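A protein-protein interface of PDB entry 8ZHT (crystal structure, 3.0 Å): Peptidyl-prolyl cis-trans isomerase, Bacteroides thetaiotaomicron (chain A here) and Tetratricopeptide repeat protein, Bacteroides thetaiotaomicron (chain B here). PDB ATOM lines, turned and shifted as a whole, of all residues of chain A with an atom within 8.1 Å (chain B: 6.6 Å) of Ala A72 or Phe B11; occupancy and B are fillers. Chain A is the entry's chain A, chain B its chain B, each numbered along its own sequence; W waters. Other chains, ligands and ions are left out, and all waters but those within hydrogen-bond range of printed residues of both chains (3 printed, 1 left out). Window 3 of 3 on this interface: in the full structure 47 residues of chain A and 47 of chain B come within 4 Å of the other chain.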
ATOM      1  N   THR A  68      14.231  29.514  -2.848  1.00  0.00           N
ATOM      2  CA  THR A  68      14.834  28.195  -2.946  1.00  0.00           C
ATOM      3  C   THR A  68      13.773  27.201  -3.398  1.00  0.00           C
ATOM      4  O   THR A  68      12.569  27.459  -3.313  1.00  0.00           O
ATOM      5  CB  THR A  68      15.441  27.700  -1.606  1.00  0.00           C
ATOM      6  OG1 THR A  68      14.409  27.101  -0.801  1.00  0.00           O
ATOM      7  CG2 THR A  68      16.116  28.834  -0.812  1.00  0.00           C
ATOM      8  N   VAL A  69      14.244  26.050  -3.871  1.00  0.00           N
ATOM      9  CA  VAL A  69      13.397  24.911  -4.170  1.00  0.00           C
ATOM     10  C   VAL A  69      13.855  23.805  -3.231  1.00  0.00           C
ATOM     11  O   VAL A  69      14.886  23.168  -3.466  1.00  0.00           O
ATOM     12  CB  VAL A  69      13.486  24.481  -5.634  1.00  0.00           C
ATOM     13  CG1 VAL A  69      12.483  23.381  -5.889  1.00  0.00           C
ATOM     14  CG2 VAL A  69      13.239  25.684  -6.558  1.00  0.00           C
ATOM     15  N   SER A  70      13.110  23.588  -2.154  1.00  0.00           N
ATOM     16  CA  SER A  70      13.536  22.652  -1.125  1.00  0.00           C
ATOM     17  C   SER A  70      13.285  21.207  -1.557  1.00  0.00           C
ATOM     18  O   SER A  70      12.557  20.926  -2.523  1.00  0.00           O
ATOM     19  CB  SER A  70      12.816  22.945   0.194  1.00  0.00           C
ATOM     20  OG  SER A  70      11.406  22.827   0.047  1.00  0.00           O
ATOM     21  N   ALA A  71      13.924  20.283  -0.832  1.00  0.00           N
ATOM     22  CA  ALA A  71      13.727  18.861  -1.098  1.00  0.00           C
ATOM     23  C   ALA A  71      12.258  18.477  -0.956  1.00  0.00           C
ATOM     24  O   ALA A  71      11.747  17.640  -1.714  1.00  0.00           O
ATOM     25  CB  ALA A  71      14.598  18.028  -0.155  1.00  0.00           C
ATOM     26  N   ALA A  72      11.560  19.095   0.004  1.00  0.00           N
ATOM     27  CA  ALA A  72      10.129  18.852   0.174  1.00  0.00           C
ATOM     28  C   ALA A  72       9.351  19.239  -1.081  1.00  0.00           C
ATOM     29  O   ALA A  72       8.499  18.478  -1.556  1.00  0.00           O
ATOM     30  CB  ALA A  72       9.611  19.617   1.396  1.00  0.00           C
ATOM     31  N   GLU A  73       9.637  20.420  -1.637  1.00  0.00           N
ATOM     32  CA  GLU A  73       8.938  20.839  -2.848  1.00  0.00           C
ATOM     33  C   GLU A  73       9.202  19.887  -4.007  1.00  0.00           C
ATOM     34  O   GLU A  73       8.296  19.599  -4.794  1.00  0.00           O
ATOM     35  CB  GLU A  73       9.333  22.262  -3.239  1.00  0.00           C
ATOM     36  CG  GLU A  73       8.338  22.865  -4.208  1.00  0.00           C
ATOM     37  CD  GLU A  73       8.704  24.260  -4.677  1.00  0.00           C
ATOM     38  OE1 GLU A  73       9.576  24.902  -4.038  1.00  0.00           O
ATOM     39  OE2 GLU A  73       8.100  24.709  -5.683  1.00  0.00           O
ATOM     40  N   ILE A  74      10.440  19.400  -4.134  1.00  0.00           N
ATOM     41  CA  ILE A  74      10.768  18.469  -5.211  1.00  0.00           C
ATOM     42  C   ILE A  74       9.951  17.190  -5.071  1.00  0.00           C
ATOM     43  O   ILE A  74       9.363  16.699  -6.045  1.00  0.00           O
ATOM     44  CB  ILE A  74      12.273  18.164  -5.221  1.00  0.00           C
ATOM     45  CG1 ILE A  74      13.076  19.411  -5.578  1.00  0.00           C
ATOM     46  CG2 ILE A  74      12.570  17.087  -6.244  1.00  0.00           C
ATOM     47  CD1 ILE A  74      12.610  20.044  -6.864  1.00  0.00           C
ATOM     48  N   GLN A  75       9.907  16.630  -3.854  1.00  0.00           N
ATOM     49  CA  GLN A  75       9.044  15.479  -3.595  1.00  0.00           C
ATOM     50  C   GLN A  75       7.601  15.780  -3.955  1.00  0.00           C
ATOM     51  O   GLN A  75       6.927  14.955  -4.583  1.00  0.00           O
ATOM     52  CB  GLN A  75       9.125  15.046  -2.126  1.00  0.00           C
ATOM     53  CG  GLN A  75      10.528  14.696  -1.633  1.00  0.00           C
ATOM     54  CD  GLN A  75      11.087  13.417  -2.242  1.00  0.00           C
ATOM     55  OE1 GLN A  75      10.539  12.881  -3.207  1.00  0.00           O
ATOM     56  NE2 GLN A  75      12.199  12.934  -1.687  1.00  0.00           N
ATOM     57  N   ASP A  76       7.106  16.958  -3.560  1.00  0.00           N
ATOM     58  CA  ASP A  76       5.741  17.344  -3.903  1.00  0.00           C
ATOM     59  C   ASP A  76       5.539  17.357  -5.415  1.00  0.00           C
ATOM     60  O   ASP A  76       4.571  16.780  -5.927  1.00  0.00           O
ATOM     61  CB  ASP A  76       5.416  18.712  -3.298  1.00  0.00           C
ATOM     62  CG  ASP A  76       3.911  18.952  -3.130  1.00  0.00           C
ATOM     63  OD1 ASP A  76       3.320  18.370  -2.188  1.00  0.00           O
ATOM     64  OD2 ASP A  76       3.332  19.758  -3.906  1.00  0.00           O
ATOM     65  N   ILE A  77       6.450  18.012  -6.147  1.00  0.00           N
ATOM     66  CA  ILE A  77       6.355  18.049  -7.608  1.00  0.00           C
ATOM     67  C   ILE A  77       6.421  16.639  -8.190  1.00  0.00           C
ATOM     68  O   ILE A  77       5.716  16.314  -9.154  1.00  0.00           O
ATOM     69  CB  ILE A  77       7.465  18.948  -8.185  1.00  0.00           C
ATOM     70  CG1 ILE A  77       7.304  20.374  -7.675  1.00  0.00           C
ATOM     71  CG2 ILE A  77       7.424  18.939  -9.701  1.00  0.00           C
ATOM     72  CD1 ILE A  77       8.337  21.349  -8.199  1.00  0.00           C
ATOM     73  N   LEU A  78       7.280  15.785  -7.624  1.00  0.00           N
ATOM     74  CA  LEU A  78       7.443  14.436  -8.154  1.00  0.00           C
ATOM     75  C   LEU A  78       6.178  13.604  -7.941  1.00  0.00           C
ATOM     76  O   LEU A  78       5.701  12.937  -8.867  1.00  0.00           O
ATOM     77  CB  LEU A  78       8.657  13.764  -7.506  1.00  0.00           C
ATOM     78  CG  LEU A  78      10.021  14.286  -7.969  1.00  0.00           C
ATOM     79  CD1 LEU A  78      11.180  13.554  -7.289  1.00  0.00           C
ATOM     80  CD2 LEU A  78      10.137  14.221  -9.489  1.00  0.00           C
ATOM     81  N   LYS A  79       5.614  13.649  -6.724  1.00  0.00           N
ATOM     82  CA  LYS A  79       4.376  12.925  -6.432  1.00  0.00           C
ATOM     83  C   LYS A  79       3.219  13.401  -7.302  1.00  0.00           C
ATOM     84  O   LYS A  79       2.308  12.621  -7.600  1.00  0.00           O
ATOM     85  CB  LYS A  79       4.005  13.074  -4.951  1.00  0.00           C
ATOM     86  CG  LYS A  79       4.964  12.409  -3.979  1.00  0.00           C
ATOM     87  CD  LYS A  79       4.395  12.413  -2.565  1.00  0.00           C
ATOM     88  CE  LYS A  79       5.488  12.646  -1.535  1.00  0.00           C
ATOM     89  NZ  LYS A  79       6.412  11.473  -1.431  1.00  0.00           N
ATOM     90  N   ARG A 145      12.056  25.562 -11.822  1.00  0.00           N
ATOM     91  CA  ARG A 145      11.165  26.001 -10.751  1.00  0.00           C
ATOM     92  C   ARG A 145      11.716  27.243 -10.051  1.00  0.00           C
ATOM     93  O   ARG A 145      10.958  28.148  -9.687  1.00  0.00           O
ATOM     94  CB  ARG A 145      10.955  24.851  -9.756  1.00  0.00           C
ATOM     95  CG  ARG A 145       9.823  25.038  -8.745  1.00  0.00           C
ATOM     96  CD  ARG A 145       8.512  25.550  -9.358  1.00  0.00           C
ATOM     97  NE  ARG A 145       7.663  26.130  -8.318  1.00  0.00           N
ATOM     98  CZ  ARG A 145       6.973  27.263  -8.425  1.00  0.00           C
ATOM     99  NH1 ARG A 145       6.980  27.976  -9.541  1.00  0.00           N
ATOM    100  NH2 ARG A 145       6.240  27.682  -7.389  1.00  0.00           N
ATOM    101  N   LYS A 149       9.690  30.739  -9.927  1.00  0.00           N
ATOM    102  CA  LYS A 149       9.340  31.426  -8.683  1.00  0.00           C
ATOM    103  C   LYS A 149       9.778  32.880  -8.735  1.00  0.00           C
ATOM    104  O   LYS A 149       9.037  33.786  -8.349  1.00  0.00           O
ATOM    105  CB  LYS A 149      10.014  30.753  -7.486  1.00  0.00           C
ATOM    106  CG  LYS A 149       9.270  29.614  -6.881  1.00  0.00           C
ATOM    107  CD  LYS A 149       9.979  29.173  -5.609  1.00  0.00           C
ATOM    108  CE  LYS A 149       9.518  27.791  -5.191  1.00  0.00           C
ATOM    109  NZ  LYS A 149      10.031  27.430  -3.828  1.00  0.00           N
ATOM    110  N   ALA B   6      11.389  26.896   7.510  1.00  0.00           N
ATOM    111  CA  ALA B   6      10.597  28.021   7.031  1.00  0.00           C
ATOM    112  C   ALA B   6      10.350  27.921   5.527  1.00  0.00           C
ATOM    113  O   ALA B   6       9.251  28.225   5.059  1.00  0.00           O
ATOM    114  CB  ALA B   6      11.303  29.341   7.370  1.00  0.00           C
ATOM    115  N   GLN B   7      11.361  27.487   4.766  1.00  0.00           N
ATOM    116  CA  GLN B   7      11.235  27.348   3.318  1.00  0.00           C
ATOM    117  C   GLN B   7      10.272  26.225   2.952  1.00  0.00           C
ATOM    118  O   GLN B   7       9.529  26.332   1.971  1.00  0.00           O
ATOM    119  CB  GLN B   7      12.610  27.080   2.717  1.00  0.00           C
ATOM    120  CG  GLN B   7      13.592  28.229   2.885  1.00  0.00           C
ATOM    121  CD  GLN B   7      13.341  29.345   1.892  1.00  0.00           C
ATOM    122  OE1 GLN B   7      12.721  29.132   0.842  1.00  0.00           O
ATOM    123  NE2 GLN B   7      13.819  30.540   2.210  1.00  0.00           N
ATOM    124  N   ALA B   8      10.269  25.136   3.730  1.00  0.00           N
ATOM    125  CA  ALA B   8       9.298  24.078   3.490  1.00  0.00           C
ATOM    126  C   ALA B   8       7.887  24.518   3.867  1.00  0.00           C
ATOM    127  O   ALA B   8       6.918  24.053   3.257  1.00  0.00           O
ATOM    128  CB  ALA B   8       9.693  22.814   4.246  1.00  0.00           C
ATOM    129  N   ALA B   9       7.740  25.415   4.848  1.00  0.00           N
ATOM    130  CA  ALA B   9       6.399  25.890   5.189  1.00  0.00           C
ATOM    131  C   ALA B   9       5.865  26.899   4.177  1.00  0.00           C
ATOM    132  O   ALA B   9       4.651  27.114   4.112  1.00  0.00           O
ATOM    133  CB  ALA B   9       6.392  26.506   6.588  1.00  0.00           C
ATOM    134  N   LEU B  10       6.742  27.499   3.378  1.00  0.00           N
ATOM    135  CA  LEU B  10       6.384  28.553   2.440  1.00  0.00           C
ATOM    136  C   LEU B  10       6.003  28.047   1.046  1.00  0.00           C
ATOM    137  O   LEU B  10       5.147  28.655   0.401  1.00  0.00           O
ATOM    138  CB  LEU B  10       7.556  29.534   2.314  1.00  0.00           C
ATOM    139  CG  LEU B  10       7.366  30.771   1.447  1.00  0.00           C
ATOM    140  CD1 LEU B  10       6.596  31.810   2.258  1.00  0.00           C
ATOM    141  CD2 LEU B  10       8.715  31.322   0.996  1.00  0.00           C
ATOM    142  N   PHE B  11       6.597  26.951   0.558  1.00  0.00           N
ATOM    143  CA  PHE B  11       6.529  26.660  -0.879  1.00  0.00           C
ATOM    144  C   PHE B  11       5.101  26.436  -1.369  1.00  0.00           C
ATOM    145  O   PHE B  11       4.785  26.792  -2.508  1.00  0.00           O
ATOM    146  CB  PHE B  11       7.443  25.478  -1.250  1.00  0.00           C
ATOM    147  CG  PHE B  11       6.840  24.096  -1.034  1.00  0.00           C
ATOM    148  CD1 PHE B  11       5.937  23.545  -1.943  1.00  0.00           C
ATOM    149  CD2 PHE B  11       7.239  23.316   0.051  1.00  0.00           C
ATOM    150  CE1 PHE B  11       5.405  22.263  -1.748  1.00  0.00           C
ATOM    151  CE2 PHE B  11       6.713  22.039   0.251  1.00  0.00           C
ATOM    152  CZ  PHE B  11       5.801  21.510  -0.650  1.00  0.00           C
ATOM    153  N   LYS B  12       4.217  25.880  -0.537  1.00  0.00           N
ATOM    154  CA  LYS B  12       2.843  25.686  -0.993  1.00  0.00           C
ATOM    155  C   LYS B  12       2.148  27.021  -1.227  1.00  0.00           C
ATOM    156  O   LYS B  12       1.326  27.151  -2.146  1.00  0.00           O
ATOM    157  CB  LYS B  12       2.052  24.849   0.014  1.00  0.00           C
ATOM    158  CG  LYS B  12       0.925  24.079  -0.619  1.00  0.00           C
ATOM    159  CD  LYS B  12       1.442  22.750  -1.150  1.00  0.00           C
ATOM    160  CE  LYS B  12       0.564  22.214  -2.271  1.00  0.00           C
ATOM    161  NZ  LYS B  12       1.184  21.013  -2.928  1.00  0.00           N
ATOM    162  N   GLY B  13       2.450  28.019  -0.390  1.00  0.00           N
ATOM    163  CA  GLY B  13       1.923  29.346  -0.637  1.00  0.00           C
ATOM    164  C   GLY B  13       2.444  29.954  -1.922  1.00  0.00           C
ATOM    165  O   GLY B  13       1.736  30.719  -2.572  1.00  0.00           O
ATOM    166  N   GLN B  14       3.681  29.629  -2.304  1.00  0.00           N
ATOM    167  CA  GLN B  14       4.213  30.141  -3.561  1.00  0.00           C
ATOM    168  C   GLN B  14       3.470  29.546  -4.748  1.00  0.00           C
ATOM    169  O   GLN B  14       3.243  30.241  -5.737  1.00  0.00           O
ATOM    170  CB  GLN B  14       5.709  29.851  -3.658  1.00  0.00           C
ATOM    171  CG  GLN B  14       6.541  30.786  -2.813  1.00  0.00           C
ATOM    172  CD  GLN B  14       7.924  30.242  -2.519  1.00  0.00           C
ATOM    173  OE1 GLN B  14       8.109  29.052  -2.263  1.00  0.00           O
ATOM    174  NE2 GLN B  14       8.911  31.121  -2.568  1.00  0.00           N
ATOM    175  N   GLU B  15       3.024  28.292  -4.631  1.00  0.00           N
ATOM    176  CA  GLU B  15       2.179  27.678  -5.658  1.00  0.00           C
ATOM    177  C   GLU B  15       0.815  28.353  -5.746  1.00  0.00           C
ATOM    178  O   GLU B  15       0.366  28.706  -6.841  1.00  0.00           O
ATOM    179  CB  GLU B  15       1.996  26.200  -5.363  1.00  0.00           C
ATOM    180  CG  GLU B  15       3.177  25.337  -5.684  1.00  0.00           C
ATOM    181  CD  GLU B  15       2.831  23.854  -5.522  1.00  0.00           C
ATOM    182  OE1 GLU B  15       1.608  23.535  -5.510  1.00  0.00           O
ATOM    183  OE2 GLU B  15       3.769  23.019  -5.404  1.00  0.00           O
ATOM    184  N   TYR B  16       0.113  28.503  -4.607  1.00  0.00           N
ATOM    185  CA  TYR B  16      -1.180  29.196  -4.630  1.00  0.00           C
ATOM    186  C   TYR B  16      -1.049  30.594  -5.225  1.00  0.00           C
ATOM    187  O   TYR B  16      -1.913  31.043  -5.993  1.00  0.00           O
ATOM    188  CB  TYR B  16      -1.770  29.321  -3.227  1.00  0.00           C
ATOM    189  CG  TYR B  16      -2.320  28.044  -2.640  1.00  0.00           C
ATOM    190  CD1 TYR B  16      -3.247  27.270  -3.342  1.00  0.00           C
ATOM    191  CD2 TYR B  16      -1.922  27.616  -1.378  1.00  0.00           C
ATOM    192  CE1 TYR B  16      -3.747  26.095  -2.809  1.00  0.00           C
ATOM    193  CE2 TYR B  16      -2.429  26.444  -0.821  1.00  0.00           C
ATOM    194  CZ  TYR B  16      -3.338  25.688  -1.541  1.00  0.00           C
ATOM    195  OH  TYR B  16      -3.834  24.527  -0.998  1.00  0.00           O
ATOM    196  N   TYR B  33      -1.003  23.781   4.862  1.00  0.00           N
ATOM    197  CA  TYR B  33      -0.346  25.051   4.555  1.00  0.00           C
ATOM    198  C   TYR B  33      -0.996  26.156   5.387  1.00  0.00           C
ATOM    199  O   TYR B  33      -2.209  26.379   5.293  1.00  0.00           O
ATOM    200  CB  TYR B  33      -0.427  25.388   3.058  1.00  0.00           C
ATOM    201  CG  TYR B  33       0.074  26.796   2.785  1.00  0.00           C
ATOM    202  CD1 TYR B  33       1.403  27.131   2.996  1.00  0.00           C
ATOM    203  CD2 TYR B  33      -0.788  27.791   2.376  1.00  0.00           C
ATOM    204  CE1 TYR B  33       1.872  28.443   2.789  1.00  0.00           C
ATOM    205  CE2 TYR B  33      -0.341  29.076   2.158  1.00  0.00           C
ATOM    206  CZ  TYR B  33       0.986  29.398   2.385  1.00  0.00           C
ATOM    207  OH  TYR B  33       1.408  30.680   2.180  1.00  0.00           O
HETATM  208  O   HOH W   1      10.338  27.685  -0.378  1.00  0.00           O
HETATM  209  O   HOH W   2      11.537  30.113  -1.537  1.00  0.00           O
HETATM  210  O   HOH W   3       6.507  26.770  -4.592  1.00  0.00           O
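OG1 of Thr A68 lies within hydrogen-bond range of OE1 of Gln B7 (3.1 Å). The side-chain amino group (NZ) of Lys A149 lies within hydrogen-bond range of the side-chain amide oxygen (OE1) of Gln B14. The side-chain carboxylate (OD2) of Asp A76 is in salt-bridge range of the side-chain amino group (NZ) of Lys B12 (2.7 Å).
NZ of Lys B12 lies within salt-bridge range of OE1 of Glu B15 (3.6 Å). OG of Ser A70 is in hydrogen-bond range of N of Glu A73 (3.4 Å). NZ of Lys A149 lies within salt-bridge range of OE1 of Glu A73 (2.6 Å). The backbone carbonyl oxygen (O) of Thr A68 sits at hydrogen-bond distance from the side-chain amino group (NZ) of Lys A149 (2.6 Å). NE of Arg A145 lies within salt-bridge range of OE2 of Glu A73 (3.0 Å).
Ala A72 touches Phe B11. Glu A73 touches Phe B11 (CG to CD1, 3.4 Å). Phe B11 touches Asp A76 (CZ to CB, 3.9 Å). Glu B15 touches Asp A76 (OE2 to OD2, 3.6 Å).
Of the printed residues of chain B, Thr A68 touches Gln B7 (3.1 Å). Of chain B, only Phe B11 (3.9 Å) comes within 4 Å of Ala A72. Of the printed residues of chain A, Gln B7 touches Thr A68. Of chain A, only Ala A72, Glu A73 and Asp A76 come within 4 Å of Phe B11. Of the printed residues of chain A, Lys B12 touches Asp A76 (2.7 Å). Printed residues of chain A within 4 Å of Glu B15: Asp A76. The nearest residue of chain B that does not touch Ala A72 is Ala B8 (4.3 Å). The nearest residue of chain A that does not touch Phe B11 is Lys A149 (4.1 Å).
Of the 14 printed residues of chain A, 5 touch a printed residue of chain B. Printed residues of chain A that touch a printed residue of chain B: Thr A68, Ala A72, Glu A73, Asp A76 and Lys A149. Printed residues of chain B that touch a printed residue of chain A: Gln B7, Phe B11, Lys B12, Gln B14 and Glu B15. Among the printed residues, Asp or Glu carboxylates within 4 Å of a Lys or Arg side-chain nitrogen of the other chain: Asp A76 with Lys B12 (2.7 Å).
Water W3 lies within hydrogen-bond range of O of Phe B11 (2.7 Å), OE2 of Glu A73 (2.8 Å) and NH2 of Arg A145 (3.0 Å). Water W1 lies within hydrogen-bond range of O of Gln B7 (2.8 Å), OE1 of Gln B14 (3.2 Å) and NZ of Lys A149 (3.5 Å). Water W2 lies within hydrogen-bond range of OE1 of Gln B7 (2.8 Å), NE2 of Gln B14 (3.0 Å) and N of Thr A68 (3.1 Å).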
